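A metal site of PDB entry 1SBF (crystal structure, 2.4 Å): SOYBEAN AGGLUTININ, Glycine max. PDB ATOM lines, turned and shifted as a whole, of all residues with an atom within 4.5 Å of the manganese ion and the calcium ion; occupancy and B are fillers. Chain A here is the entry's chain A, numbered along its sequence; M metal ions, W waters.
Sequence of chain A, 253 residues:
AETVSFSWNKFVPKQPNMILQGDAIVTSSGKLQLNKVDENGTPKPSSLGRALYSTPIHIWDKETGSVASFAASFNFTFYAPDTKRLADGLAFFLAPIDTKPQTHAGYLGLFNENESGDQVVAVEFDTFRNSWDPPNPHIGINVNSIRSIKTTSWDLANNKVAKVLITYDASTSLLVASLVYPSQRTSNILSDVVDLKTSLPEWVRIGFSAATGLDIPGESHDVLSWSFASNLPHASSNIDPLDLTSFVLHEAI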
ATOM      1  N   GLU A 124      19.637  -1.113 -19.455  1.00  0.00           N
ATOM      2  CA  GLU A 124      19.450  -2.482 -19.935  1.00  0.00           C
ATOM      3  C   GLU A 124      18.838  -3.431 -18.947  1.00  0.00           C
ATOM      4  O   GLU A 124      19.074  -3.353 -17.749  1.00  0.00           O
ATOM      5  CB  GLU A 124      20.818  -3.054 -20.376  1.00  0.00           C
ATOM      6  CG  GLU A 124      21.686  -3.567 -19.199  1.00  0.00           C
ATOM      7  CD  GLU A 124      22.889  -4.373 -19.635  1.00  0.00           C
ATOM      8  OE1 GLU A 124      23.359  -4.000 -20.796  1.00  0.00           O
ATOM      9  OE2 GLU A 124      23.296  -5.366 -19.064  1.00  0.00           O
ATOM     10  N   ASP A 126      19.310  -7.224 -18.847  1.00  0.00           N
ATOM     11  CA  ASP A 126      20.149  -8.157 -19.564  1.00  0.00           C
ATOM     12  C   ASP A 126      20.031  -9.603 -19.087  1.00  0.00           C
ATOM     13  O   ASP A 126      20.348  -9.902 -17.941  1.00  0.00           O
ATOM     14  CB  ASP A 126      21.595  -7.607 -19.499  1.00  0.00           C
ATOM     15  CG  ASP A 126      22.538  -8.478 -20.259  1.00  0.00           C
ATOM     16  OD1 ASP A 126      22.214  -9.552 -20.721  1.00  0.00           O
ATOM     17  OD2 ASP A 126      23.651  -7.859 -20.560  1.00  0.00           O
ATOM     18  N   PHE A 128      21.473 -12.429 -20.676  1.00  0.00           N
ATOM     19  CA  PHE A 128      22.505 -13.329 -21.064  1.00  0.00           C
ATOM     20  C   PHE A 128      23.888 -12.818 -20.741  1.00  0.00           C
ATOM     21  O   PHE A 128      24.246 -11.699 -21.109  1.00  0.00           O
ATOM     22  CB  PHE A 128      22.381 -13.604 -22.548  1.00  0.00           C
ATOM     23  CG  PHE A 128      23.321 -14.709 -22.891  1.00  0.00           C
ATOM     24  CD1 PHE A 128      22.974 -16.030 -22.617  1.00  0.00           C
ATOM     25  CD2 PHE A 128      24.614 -14.434 -23.337  1.00  0.00           C
ATOM     26  CE1 PHE A 128      23.830 -17.078 -22.925  1.00  0.00           C
ATOM     27  CE2 PHE A 128      25.502 -15.454 -23.641  1.00  0.00           C
ATOM     28  CZ  PHE A 128      25.111 -16.779 -23.423  1.00  0.00           C
ATOM     29  N   ARG A 129      24.667 -13.652 -20.054  1.00  0.00           N
ATOM     30  CA  ARG A 129      26.036 -13.300 -19.659  1.00  0.00           C
ATOM     31  C   ARG A 129      26.996 -13.304 -20.828  1.00  0.00           C
ATOM     32  O   ARG A 129      27.379 -14.354 -21.299  1.00  0.00           O
ATOM     33  CB  ARG A 129      26.587 -14.217 -18.557  1.00  0.00           C
ATOM     34  N   ASN A 130      27.436 -12.126 -21.266  1.00  0.00           N
ATOM     35  CA  ASN A 130      28.474 -12.078 -22.258  1.00  0.00           C
ATOM     36  C   ASN A 130      29.762 -11.902 -21.517  1.00  0.00           C
ATOM     37  O   ASN A 130      29.751 -11.828 -20.284  1.00  0.00           O
ATOM     38  CB  ASN A 130      28.228 -10.997 -23.322  1.00  0.00           C
ATOM     39  CG  ASN A 130      26.789 -11.100 -23.807  1.00  0.00           C
ATOM     40  OD1 ASN A 130      25.850 -10.553 -23.202  1.00  0.00           O
ATOM     41  ND2 ASN A 130      26.574 -11.981 -24.780  1.00  0.00           N
ATOM     42  N   TRP A 132      31.662  -9.490 -21.072  1.00  0.00           N
ATOM     43  CA  TRP A 132      31.757  -8.262 -20.302  1.00  0.00           C
ATOM     44  C   TRP A 132      30.815  -8.206 -19.116  1.00  0.00           C
ATOM     45  O   TRP A 132      30.899  -7.261 -18.331  1.00  0.00           O
ATOM     46  CB  TRP A 132      31.514  -7.025 -21.172  1.00  0.00           C
ATOM     47  CG  TRP A 132      30.225  -7.132 -21.928  1.00  0.00           C
ATOM     48  CD1 TRP A 132      28.993  -6.808 -21.462  1.00  0.00           C
ATOM     49  CD2 TRP A 132      30.037  -7.693 -23.221  1.00  0.00           C
ATOM     50  NE1 TRP A 132      28.042  -7.111 -22.394  1.00  0.00           N
ATOM     51  CE2 TRP A 132      28.656  -7.632 -23.483  1.00  0.00           C
ATOM     52  CE3 TRP A 132      30.916  -8.184 -24.183  1.00  0.00           C
ATOM     53  CZ2 TRP A 132      28.133  -8.048 -24.707  1.00  0.00           C
ATOM     54  CZ3 TRP A 132      30.400  -8.588 -25.396  1.00  0.00           C
ATOM     55  CH2 TRP A 132      29.011  -8.542 -25.636  1.00  0.00           C
ATOM     56  N   ASP A 133      29.948  -9.215 -19.002  1.00  0.00           N
ATOM     57  CA  ASP A 133      28.835  -9.232 -18.064  1.00  0.00           C
ATOM     58  C   ASP A 133      29.141  -9.823 -16.729  1.00  0.00           C
ATOM     59  O   ASP A 133      30.026 -10.667 -16.608  1.00  0.00           O
ATOM     60  CB  ASP A 133      27.647  -9.991 -18.676  1.00  0.00           C
ATOM     61  CG  ASP A 133      26.847  -9.151 -19.631  1.00  0.00           C
ATOM     62  OD1 ASP A 133      26.527  -7.971 -19.134  1.00  0.00           O
ATOM     63  OD2 ASP A 133      26.570  -9.518 -20.759  1.00  0.00           O
ATOM     64  N   HIS A 138      20.573  -9.023 -14.976  1.00  0.00           N
ATOM     65  CA  HIS A 138      20.878  -7.794 -14.285  1.00  0.00           C
ATOM     66  C   HIS A 138      20.233  -6.643 -14.995  1.00  0.00           C
ATOM     67  O   HIS A 138      19.709  -6.763 -16.110  1.00  0.00           O
ATOM     68  CB  HIS A 138      22.422  -7.589 -14.196  1.00  0.00           C
ATOM     69  CG  HIS A 138      23.136  -7.725 -15.530  1.00  0.00           C
ATOM     70  ND1 HIS A 138      23.372  -8.963 -16.130  1.00  0.00           N
ATOM     71  CD2 HIS A 138      23.624  -6.767 -16.379  1.00  0.00           C
ATOM     72  CE1 HIS A 138      24.000  -8.730 -17.281  1.00  0.00           C
ATOM     73  NE2 HIS A 138      24.203  -7.424 -17.451  1.00  0.00           N
ATOM     74  N   SER A 148      28.529  -2.182 -19.127  1.00  0.00           N
ATOM     75  CA  SER A 148      27.832  -1.315 -18.163  1.00  0.00           C
ATOM     76  C   SER A 148      28.697  -0.623 -17.107  1.00  0.00           C
ATOM     77  O   SER A 148      29.536  -1.262 -16.496  1.00  0.00           O
ATOM     78  CB  SER A 148      26.618  -1.986 -17.528  1.00  0.00           C
ATOM     79  OG  SER A 148      25.838  -2.637 -18.520  1.00  0.00           O
HETATM   80 MN    MN M   1      24.887  -6.660 -19.444  1.00  0.00          MN
HETATM   81 CA    CA M   2      24.407  -9.632 -21.869  1.00  0.00          CA
HETATM   82  O   HOH W   1      25.474  -5.808 -21.240  1.00  0.00           O
HETATM   83  O   HOH W   2      25.110  -7.778 -23.109  1.00  0.00           O
HETATM   84  O   HOH W   3      26.058  -5.368 -18.489  1.00  0.00           O
HETATM   85  O   HOH W   4      22.891 -10.322 -23.128  1.00  0.00           O
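NE1 of Trp 132 sits close to OD2 of Asp 133 (3.3 Å).
Within 4 Å of the manganese ion: Glu 124, Asp 126, Asp 133 and His 138. The nearest printed residue that does not touch the manganese ion is Ser 148 (4.2 Å).
Water W3 is bound to the manganese ion, at 2.0 Å. The manganese ion is bound by OD2 of Asp 126 (2.1 Å). The manganese ion is bound by water W1 (2.1 Å). The side-chain carboxylate (OE2) of Glu 124 is bound to the manganese ion (2.1 Å). The manganese ion is bound by the side-chain carboxylate (OD1) of Asp 133. NE2 of His 138 is bound to the manganese ion, at 2.2 Å. The manganese ion has six donor atoms within binding distance.
Water W4 binds the calcium ion (2.1 Å). OD1 of Asn 130 is bound to the calcium ion, at 2.2 Å. O of Phe 128 is bound to the calcium ion (2.2 Å). The calcium ion is bound by the side-chain carboxylate (OD2) of Asp 126 (2.3 Å). The calcium ion is bound by water W2 (2.3 Å). The calcium ion is bound by the side-chain carboxylate (OD2) of Asp 133 (2.4 Å). OD1 of Asp 126 binds the calcium ion, 2.5 Å away.
Water W1 bridges the side-chain carboxylate (OE1) of Glu 124 (2.8 Å) and the indole nitrogen (NE1) of Trp 132 (3.1 Å).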
